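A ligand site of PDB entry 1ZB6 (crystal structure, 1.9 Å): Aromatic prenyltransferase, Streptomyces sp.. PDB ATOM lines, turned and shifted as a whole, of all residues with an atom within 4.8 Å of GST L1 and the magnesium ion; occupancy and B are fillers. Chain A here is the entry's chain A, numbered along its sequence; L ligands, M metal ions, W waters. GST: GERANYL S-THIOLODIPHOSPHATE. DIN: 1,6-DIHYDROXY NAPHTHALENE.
ND2 of Asn 173 sits at hydrogen-bond distance from O1A of GST L1, at 2.6 Å. An oxygen (O2A) of GST L1 is in salt-bridge range of the side-chain amino group of Lys 119, 2.6 Å away. OH of Tyr 216 sits at hydrogen-bond distance from O2B of GST L1. A sulfur (S1) of GST L1 lies close to the side-chain hydroxyl (OH) of Tyr 121, at 3.7 Å. The guanidinium group (NH2) of Arg 228 is in salt-bridge range of an oxygen (O1A) of GST L1 (2.8 Å). NZ of Lys 284 is in salt-bridge range of O2B of GST L1, at 3.0 Å. The side-chain hydroxyl of Tyr 175 sits close to a sulfur (S1) of GST L1 (3.5 Å).
OD1 of Asp 62 is in salt-bridge range of NZ of Lys 118 (3.3 Å). The side-chain amide nitrogen (ND2) of Asn 173 sits at hydrogen-bond distance from the side-chain hydroxyl (OH) of Tyr 175 (3.1 Å). The side-chain amino group of Lys 119 lies within hydrogen-bond range of the side-chain hydroxyl of Tyr 121. The side-chain hydroxyl of Tyr 175 is in hydrogen-bond range of the side-chain amino group of Lys 119. N of Asp 110 lies within hydrogen-bond range of O of Lys 119. The backbone NH of Tyr 121 lies within hydrogen-bond range of the backbone carbonyl oxygen of Ala 108 (2.8 Å). OG of Ser 66 is in hydrogen-bond range of N of Val 47 (2.9 Å). The backbone NH of Lys 118 lies within hydrogen-bond range of the backbone carbonyl oxygen of Asp 110, 3.0 Å away.
Merely in contact with GST L1: Val 47 (3.4 Å), Ser 64 (3.6 Å), Asp 110 (3.9 Å), Phe 123 (3.6 Å), Met 162 (3.7 Å) and Thr 218 (3.9 Å). Hydrophobic or aromatic side chains that line GST L1: Val 47, Tyr 121, Phe 123, Met 162, Tyr 175 and Tyr 216. Within 4 Å of GST L1: Val 47, Ser 64, Asp 110, Lys 119, Tyr 121, Phe 123, Met 162, Asn 173, Tyr 175, Tyr 216, Thr 218, Arg 228 and Lys 284. Along chain A the residues within 4 Å of GST L1 span positions 47 to 284.
Merely in contact with the magnesium ion: Lys 118 (3.8 Å). The nearest printed residue that does not touch the magnesium ion is Asp 110 (4.4 Å).
The magnesium ion is bound by water W5 (2.0 Å), an oxygen (O3B) of GST L1 (2.1 Å), the side-chain carboxylate (OD2) of Asp 62 (2.2 Å), water W9 (2.2 Å) and water W8 (2.3 Å). The magnesium ion has five donor atoms within binding distance.
Water W9 lies within hydrogen-bond range of the side-chain amino group of Lys 118 (3.1 Å), the side-chain carboxylate of Asp 110 (3.1 Å) and an oxygen (O2A) of GST L1 (3.2 Å). Water W7 bridges O3A of GST L1 and NH2 of Arg 228. Water W3 lies within hydrogen-bond range of O1A of GST L1 (2.8 Å), NE of Arg 228 (2.9 Å) and NZ of Lys 284 (2.9 Å). Water W1 bridges an oxygen (O1A) of GST L1 and the side-chain amide oxygen (OD1) of Asn 173. Water W6 bridges NZ of Lys 118 (2.9 Å) and O2A of GST L1 (3.3 Å).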
ATOM      1  N   VAL A  47      15.000 -13.021   7.389  1.00  0.00           N
ATOM      2  CA  VAL A  47      13.610 -13.333   7.690  1.00  0.00           C
ATOM      3  C   VAL A  47      12.860 -12.027   7.871  1.00  0.00           C
ATOM      4  O   VAL A  47      13.238 -11.201   8.700  1.00  0.00           O
ATOM      5  CB  VAL A  47      13.484 -14.174   8.991  1.00  0.00           C
ATOM      6  CG1 VAL A  47      12.024 -14.505   9.244  1.00  0.00           C
ATOM      7  CG2 VAL A  47      14.297 -15.457   8.859  1.00  0.00           C
ATOM      8  N   VAL A  49       8.821 -10.490   8.153  1.00  0.00           N
ATOM      9  CA  VAL A  49       7.412 -10.817   8.327  1.00  0.00           C
ATOM     10  C   VAL A  49       6.560  -9.557   8.407  1.00  0.00           C
ATOM     11  O   VAL A  49       6.986  -8.537   8.943  1.00  0.00           O
ATOM     12  CB  VAL A  49       7.186 -11.631   9.620  1.00  0.00           C
ATOM     13  CG1 VAL A  49       5.805 -12.241   9.627  1.00  0.00           C
ATOM     14  CG2 VAL A  49       8.252 -12.696   9.761  1.00  0.00           C
ATOM     15  N   ASP A  62       2.584  -4.734  11.777  1.00  0.00           N
ATOM     16  CA  ASP A  62       3.897  -4.933  12.357  1.00  0.00           C
ATOM     17  C   ASP A  62       4.835  -5.569  11.352  1.00  0.00           C
ATOM     18  O   ASP A  62       4.399  -6.348  10.496  1.00  0.00           O
ATOM     19  CB  ASP A  62       3.802  -5.850  13.579  1.00  0.00           C
ATOM     20  CG  ASP A  62       3.428  -5.119  14.852  1.00  0.00           C
ATOM     21  OD1 ASP A  62       3.326  -3.873  14.816  1.00  0.00           O
ATOM     22  OD2 ASP A  62       3.232  -5.781  15.890  1.00  0.00           O
ATOM     23  N   SER A  64       8.625  -7.556  11.269  1.00  0.00           N
ATOM     24  CA  SER A  64       9.700  -8.181  12.033  1.00  0.00           C
ATOM     25  C   SER A  64      10.861  -8.442  11.076  1.00  0.00           C
ATOM     26  O   SER A  64      10.664  -8.955   9.981  1.00  0.00           O
ATOM     27  CB  SER A  64       9.232  -9.501  12.635  1.00  0.00           C
ATOM     28  OG  SER A  64       8.057  -9.338  13.391  1.00  0.00           O
ATOM     29  N   ILE A  65      12.068  -8.096  11.501  1.00  0.00           N
ATOM     30  CA  ILE A  65      13.244  -8.286  10.666  1.00  0.00           C
ATOM     31  C   ILE A  65      14.390  -8.909  11.450  1.00  0.00           C
ATOM     32  O   ILE A  65      14.775  -8.418  12.507  1.00  0.00           O
ATOM     33  CB  ILE A  65      13.701  -6.924  10.072  1.00  0.00           C
ATOM     34  CG1 ILE A  65      12.597  -6.370   9.157  1.00  0.00           C
ATOM     35  CG2 ILE A  65      15.001  -7.084   9.306  1.00  0.00           C
ATOM     36  CD1 ILE A  65      12.822  -4.941   8.724  1.00  0.00           C
ATOM     37  N   SER A  66      14.937  -9.996  10.921  1.00  0.00           N
ATOM     38  CA  SER A  66      16.041 -10.677  11.585  1.00  0.00           C
ATOM     39  C   SER A  66      17.297  -9.815  11.500  1.00  0.00           C
ATOM     40  O   SER A  66      17.459  -9.039  10.557  1.00  0.00           O
ATOM     41  CB  SER A  66      16.301 -12.030  10.926  1.00  0.00           C
ATOM     42  OG  SER A  66      16.487 -11.860   9.536  1.00  0.00           O
ATOM     43  N   ALA A 108      16.557  -9.895  16.276  1.00  0.00           N
ATOM     44  CA  ALA A 108      15.491  -9.468  15.389  1.00  0.00           C
ATOM     45  C   ALA A 108      14.882  -8.210  15.990  1.00  0.00           C
ATOM     46  O   ALA A 108      15.009  -7.960  17.195  1.00  0.00           O
ATOM     47  CB  ALA A 108      14.435 -10.553  15.242  1.00  0.00           C
ATOM     48  N   ASP A 110      11.361  -5.429  15.763  1.00  0.00           N
ATOM     49  CA  ASP A 110       9.975  -5.340  15.370  1.00  0.00           C
ATOM     50  C   ASP A 110       9.569  -3.879  15.358  1.00  0.00           C
ATOM     51  O   ASP A 110       9.994  -3.096  16.205  1.00  0.00           O
ATOM     52  CB  ASP A 110       9.155  -6.134  16.387  1.00  0.00           C
ATOM     53  CG  ASP A 110       8.737  -7.492  15.886  1.00  0.00           C
ATOM     54  OD1 ASP A 110       9.428  -8.037  15.001  1.00  0.00           O
ATOM     55  OD2 ASP A 110       7.708  -7.996  16.375  1.00  0.00           O
ATOM     56  N   LYS A 118       9.723  -0.828  18.090  1.00  0.00           N
ATOM     57  CA  LYS A 118       9.083  -1.108  19.370  1.00  0.00           C
ATOM     58  C   LYS A 118       9.646  -2.304  20.133  1.00  0.00           C
ATOM     59  O   LYS A 118       9.494  -2.375  21.356  1.00  0.00           O
ATOM     60  CB  LYS A 118       7.566  -1.267  19.177  1.00  0.00           C
ATOM     61  CG  LYS A 118       7.143  -2.404  18.265  1.00  0.00           C
ATOM     62  CD  LYS A 118       5.644  -2.685  18.438  1.00  0.00           C
ATOM     63  CE  LYS A 118       5.211  -3.935  17.683  1.00  0.00           C
ATOM     64  NZ  LYS A 118       3.817  -4.336  18.046  1.00  0.00           N
ATOM     65  N   LYS A 119      10.302  -3.238  19.449  1.00  0.00           N
ATOM     66  CA  LYS A 119      10.871  -4.390  20.156  1.00  0.00           C
ATOM     67  C   LYS A 119      12.028  -5.128  19.494  1.00  0.00           C
ATOM     68  O   LYS A 119      12.282  -5.016  18.282  1.00  0.00           O
ATOM     69  CB  LYS A 119       9.754  -5.386  20.508  1.00  0.00           C
ATOM     70  CG  LYS A 119       8.866  -5.830  19.382  1.00  0.00           C
ATOM     71  CD  LYS A 119       7.673  -6.710  19.846  1.00  0.00           C
ATOM     72  CE  LYS A 119       8.130  -7.989  20.543  1.00  0.00           C
ATOM     73  NZ  LYS A 119       7.156  -9.104  20.458  1.00  0.00           N
ATOM     74  N   TYR A 121      14.391  -8.998  19.703  1.00  0.00           N
ATOM     75  CA  TYR A 121      14.264 -10.410  20.007  1.00  0.00           C
ATOM     76  C   TYR A 121      15.662 -10.982  20.216  1.00  0.00           C
ATOM     77  O   TYR A 121      16.623 -10.537  19.591  1.00  0.00           O
ATOM     78  CB  TYR A 121      13.618 -11.186  18.848  1.00  0.00           C
ATOM     79  CG  TYR A 121      12.181 -10.847  18.557  1.00  0.00           C
ATOM     80  CD1 TYR A 121      11.834  -9.687  17.876  1.00  0.00           C
ATOM     81  CD2 TYR A 121      11.163 -11.703  18.951  1.00  0.00           C
ATOM     82  CE1 TYR A 121      10.507  -9.378  17.603  1.00  0.00           C
ATOM     83  CE2 TYR A 121       9.838 -11.415  18.689  1.00  0.00           C
ATOM     84  CZ  TYR A 121       9.515 -10.255  18.015  1.00  0.00           C
ATOM     85  OH  TYR A 121       8.195  -9.962  17.792  1.00  0.00           O
ATOM     86  N   PHE A 123      17.383 -14.694  20.091  1.00  0.00           N
ATOM     87  CA  PHE A 123      17.164 -16.096  19.767  1.00  0.00           C
ATOM     88  C   PHE A 123      18.272 -16.952  20.358  1.00  0.00           C
ATOM     89  O   PHE A 123      19.426 -16.531  20.427  1.00  0.00           O
ATOM     90  CB  PHE A 123      17.160 -16.332  18.246  1.00  0.00           C
ATOM     91  CG  PHE A 123      15.980 -15.767  17.545  1.00  0.00           C
ATOM     92  CD1 PHE A 123      15.862 -14.393  17.355  1.00  0.00           C
ATOM     93  CD2 PHE A 123      14.984 -16.607  17.048  1.00  0.00           C
ATOM     94  CE1 PHE A 123      14.748 -13.858  16.678  1.00  0.00           C
ATOM     95  CE2 PHE A 123      13.873 -16.086  16.362  1.00  0.00           C
ATOM     96  CZ  PHE A 123      13.763 -14.716  16.171  1.00  0.00           C
ATOM     97  N   MET A 162      13.373 -18.323  22.206  1.00  0.00           N
ATOM     98  CA  MET A 162      13.711 -16.914  22.094  1.00  0.00           C
ATOM     99  C   MET A 162      12.822 -16.059  23.006  1.00  0.00           C
ATOM    100  O   MET A 162      11.806 -16.515  23.488  1.00  0.00           O
ATOM    101  CB  MET A 162      13.544 -16.415  20.662  1.00  0.00           C
ATOM    102  CG  MET A 162      12.105 -16.088  20.302  1.00  0.00           C
ATOM    103  SD  MET A 162      11.475 -17.057  18.937  1.00  0.00           S
ATOM    104  CE  MET A 162      10.853 -15.725  17.894  1.00  0.00           C
ATOM    105  N   ASN A 173       8.051 -11.374  26.170  1.00  0.00           N
ATOM    106  CA  ASN A 173       7.401 -12.598  25.700  1.00  0.00           C
ATOM    107  C   ASN A 173       8.413 -13.742  25.818  1.00  0.00           C
ATOM    108  O   ASN A 173       9.583 -13.562  25.494  1.00  0.00           O
ATOM    109  CB  ASN A 173       6.985 -12.482  24.226  1.00  0.00           C
ATOM    110  CG  ASN A 173       5.747 -11.625  24.022  1.00  0.00           C
ATOM    111  OD1 ASN A 173       5.140 -11.174  24.995  1.00  0.00           O
ATOM    112  ND2 ASN A 173       5.361 -11.406  22.756  1.00  0.00           N
ATOM    113  N   TYR A 175       9.032 -17.299  24.281  1.00  0.00           N
ATOM    114  CA  TYR A 175       8.572 -18.224  23.251  1.00  0.00           C
ATOM    115  C   TYR A 175       9.015 -19.648  23.558  1.00  0.00           C
ATOM    116  O   TYR A 175      10.134 -20.044  23.233  1.00  0.00           O
ATOM    117  CB  TYR A 175       9.077 -17.770  21.871  1.00  0.00           C
ATOM    118  CG  TYR A 175       8.582 -16.383  21.464  1.00  0.00           C
ATOM    119  CD1 TYR A 175       9.228 -15.229  21.911  1.00  0.00           C
ATOM    120  CD2 TYR A 175       7.448 -16.233  20.668  1.00  0.00           C
ATOM    121  CE1 TYR A 175       8.741 -13.947  21.575  1.00  0.00           C
ATOM    122  CE2 TYR A 175       6.963 -14.972  20.344  1.00  0.00           C
ATOM    123  CZ  TYR A 175       7.600 -13.836  20.795  1.00  0.00           C
ATOM    124  OH  TYR A 175       7.078 -12.602  20.469  1.00  0.00           O
ATOM    125  N   TYR A 216       3.487 -18.633  23.662  1.00  0.00           N
ATOM    126  CA  TYR A 216       4.147 -17.548  24.389  1.00  0.00           C
ATOM    127  C   TYR A 216       3.327 -16.643  25.275  1.00  0.00           C
ATOM    128  O   TYR A 216       2.361 -16.023  24.840  1.00  0.00           O
ATOM    129  CB  TYR A 216       4.995 -16.652  23.448  1.00  0.00           C
ATOM    130  CG  TYR A 216       4.323 -16.055  22.216  1.00  0.00           C
ATOM    131  CD1 TYR A 216       4.063 -14.685  22.110  1.00  0.00           C
ATOM    132  CD2 TYR A 216       4.055 -16.853  21.102  1.00  0.00           C
ATOM    133  CE1 TYR A 216       3.557 -14.121  20.907  1.00  0.00           C
ATOM    134  CE2 TYR A 216       3.568 -16.320  19.910  1.00  0.00           C
ATOM    135  CZ  TYR A 216       3.325 -14.966  19.823  1.00  0.00           C
ATOM    136  OH  TYR A 216       2.854 -14.465  18.621  1.00  0.00           O
ATOM    137  N   THR A 218       2.953 -13.325  27.898  1.00  0.00           N
ATOM    138  CA  THR A 218       3.514 -11.980  27.982  1.00  0.00           C
ATOM    139  C   THR A 218       3.556 -11.600  29.471  1.00  0.00           C
ATOM    140  O   THR A 218       2.553 -11.748  30.173  1.00  0.00           O
ATOM    141  CB  THR A 218       2.636 -10.939  27.244  1.00  0.00           C
ATOM    142  OG1 THR A 218       2.546 -11.277  25.849  1.00  0.00           O
ATOM    143  CG2 THR A 218       3.255  -9.536  27.373  1.00  0.00           C
ATOM    144  N   ARG A 228      -1.158 -11.962  28.821  1.00  0.00           N
ATOM    145  CA  ARG A 228      -1.862 -12.705  27.800  1.00  0.00           C
ATOM    146  C   ARG A 228      -1.032 -13.924  27.394  1.00  0.00           C
ATOM    147  O   ARG A 228       0.138 -14.033  27.773  1.00  0.00           O
ATOM    148  CB  ARG A 228      -2.153 -11.811  26.579  1.00  0.00           C
ATOM    149  CG  ARG A 228      -0.920 -11.172  25.962  1.00  0.00           C
ATOM    150  CD  ARG A 228      -1.274 -10.164  24.871  1.00  0.00           C
ATOM    151  NE  ARG A 228      -0.071  -9.681  24.193  1.00  0.00           N
ATOM    152  CZ  ARG A 228       0.646  -8.640  24.590  1.00  0.00           C
ATOM    153  NH1 ARG A 228       0.272  -7.935  25.662  1.00  0.00           N
ATOM    154  NH2 ARG A 228       1.752  -8.328  23.947  1.00  0.00           N
ATOM    155  N   LYS A 284      -4.127 -13.481  15.118  1.00  0.00           N
ATOM    156  CA  LYS A 284      -2.999 -12.819  14.463  1.00  0.00           C
ATOM    157  C   LYS A 284      -2.515 -13.614  13.262  1.00  0.00           C
ATOM    158  O   LYS A 284      -2.700 -14.827  13.197  1.00  0.00           O
ATOM    159  CB  LYS A 284      -1.878 -12.602  15.486  1.00  0.00           C
ATOM    160  CG  LYS A 284      -2.314 -11.705  16.639  1.00  0.00           C
ATOM    161  CD  LYS A 284      -1.200 -11.365  17.629  1.00  0.00           C
ATOM    162  CE  LYS A 284      -0.810 -12.545  18.499  1.00  0.00           C
ATOM    163  NZ  LYS A 284       0.091 -12.141  19.628  1.00  0.00           N
ATOM    164  N   GLN A 295      12.398 -21.878   8.491  1.00  0.00           N
ATOM    165  CA  GLN A 295      10.958 -21.930   8.284  1.00  0.00           C
ATOM    166  C   GLN A 295      10.590 -23.143   7.413  1.00  0.00           C
ATOM    167  O   GLN A 295       9.562 -23.789   7.632  1.00  0.00           O
ATOM    168  CB  GLN A 295      10.467 -20.638   7.621  1.00  0.00           C
ATOM    169  CG  GLN A 295      10.470 -19.422   8.559  1.00  0.00           C
ATOM    170  CD  GLN A 295      11.871 -19.011   8.998  1.00  0.00           C
ATOM    171  OE1 GLN A 295      12.058 -18.544  10.130  1.00  0.00           O
ATOM    172  NE2 GLN A 295      12.850 -19.179   8.120  1.00  0.00           N
HETATM  173  PA  GST L   1       3.262  -9.498  20.813  1.00  0.00           P
HETATM  174  O1A GST L   1       3.240  -9.985  22.223  1.00  0.00           O
HETATM  175  O2A GST L   1       4.532  -8.801  20.489  1.00  0.00           O
HETATM  176  O3A GST L   1       2.077  -8.651  20.521  1.00  0.00           O
HETATM  177  O1B GST L   1       3.155 -10.807  19.892  1.00  0.00           O
HETATM  178  PB  GST L   1       3.377 -10.971  18.327  1.00  0.00           P
HETATM  179  O2B GST L   1       2.449 -11.987  17.737  1.00  0.00           O
HETATM  180  O3B GST L   1       3.173  -9.678  17.590  1.00  0.00           O
HETATM  181  S1  GST L   1       4.871 -11.491  17.977  1.00  0.00           S
HETATM  182  C1  GST L   1       5.188 -12.075  16.728  1.00  0.00           C
HETATM  183  C2  GST L   1       6.627 -11.781  16.339  1.00  0.00           C
HETATM  184  C3  GST L   1       7.587 -12.700  16.125  1.00  0.00           C
HETATM  185  C10 GST L   1       7.729 -13.940  16.979  1.00  0.00           C
HETATM  186  C4  GST L   1       8.613 -12.521  15.040  1.00  0.00           C
HETATM  187  C5  GST L   1       9.554 -13.738  14.942  1.00  0.00           C
HETATM  188  C6  GST L   1      10.924 -13.360  14.453  1.00  0.00           C
HETATM  189  C7  GST L   1      11.493 -13.716  13.283  1.00  0.00           C
HETATM  190  C9  GST L   1      11.966 -15.131  13.046  1.00  0.00           C
HETATM  191  C8  GST L   1      11.733 -12.793  12.119  1.00  0.00           C
HETATM  192  C1  DIN L   2       6.403 -16.916  15.938  1.00  0.00           C
HETATM  193  C2  DIN L   2       5.478 -15.998  15.384  1.00  0.00           C
HETATM  194  C3  DIN L   2       5.700 -15.482  14.123  1.00  0.00           C
HETATM  195  C4  DIN L   2       6.847 -15.848  13.362  1.00  0.00           C
HETATM  196  C5  DIN L   2       7.747 -16.745  13.898  1.00  0.00           C
HETATM  197  C6  DIN L   2       8.456 -18.225  15.788  1.00  0.00           C
HETATM  198  C7  DIN L   2       7.086 -18.347  17.776  1.00  0.00           C
HETATM  199  C8  DIN L   2       6.196 -17.455  17.239  1.00  0.00           C
HETATM  200  O1  DIN L   2       9.612 -18.669  15.177  1.00  0.00           O
HETATM  201  O2  DIN L   2       4.766 -14.593  13.634  1.00  0.00           O
HETATM  202  C9  DIN L   2       8.236 -18.740  17.059  1.00  0.00           C
HETATM  203  C10 DIN L   2       7.556 -17.294  15.188  1.00  0.00           C
HETATM  204 MG    MG M   1       3.366  -7.814  16.606  1.00  0.00          MG
HETATM  205  O   HOH W   1       5.382  -8.245  23.707  1.00  0.00           O
HETATM  206  O   HOH W   2      -0.438  -8.350  20.291  1.00  0.00           O
HETATM  207  O   HOH W   3       0.998 -11.623  22.372  1.00  0.00           O
HETATM  208  O   HOH W   4       1.877 -12.180  14.844  1.00  0.00           O
HETATM  209  O   HOH W   5       1.992  -7.380  18.036  1.00  0.00           O
HETATM  210  O   HOH W   6       4.296  -5.507  20.671  1.00  0.00           O
HETATM  211  O   HOH W   7       1.696  -6.288  21.711  1.00  0.00           O
HETATM  212  O   HOH W   8       5.023  -8.568  15.258  1.00  0.00           O
HETATM  213  O   HOH W   9       5.101  -7.120  17.767  1.00  0.00           O
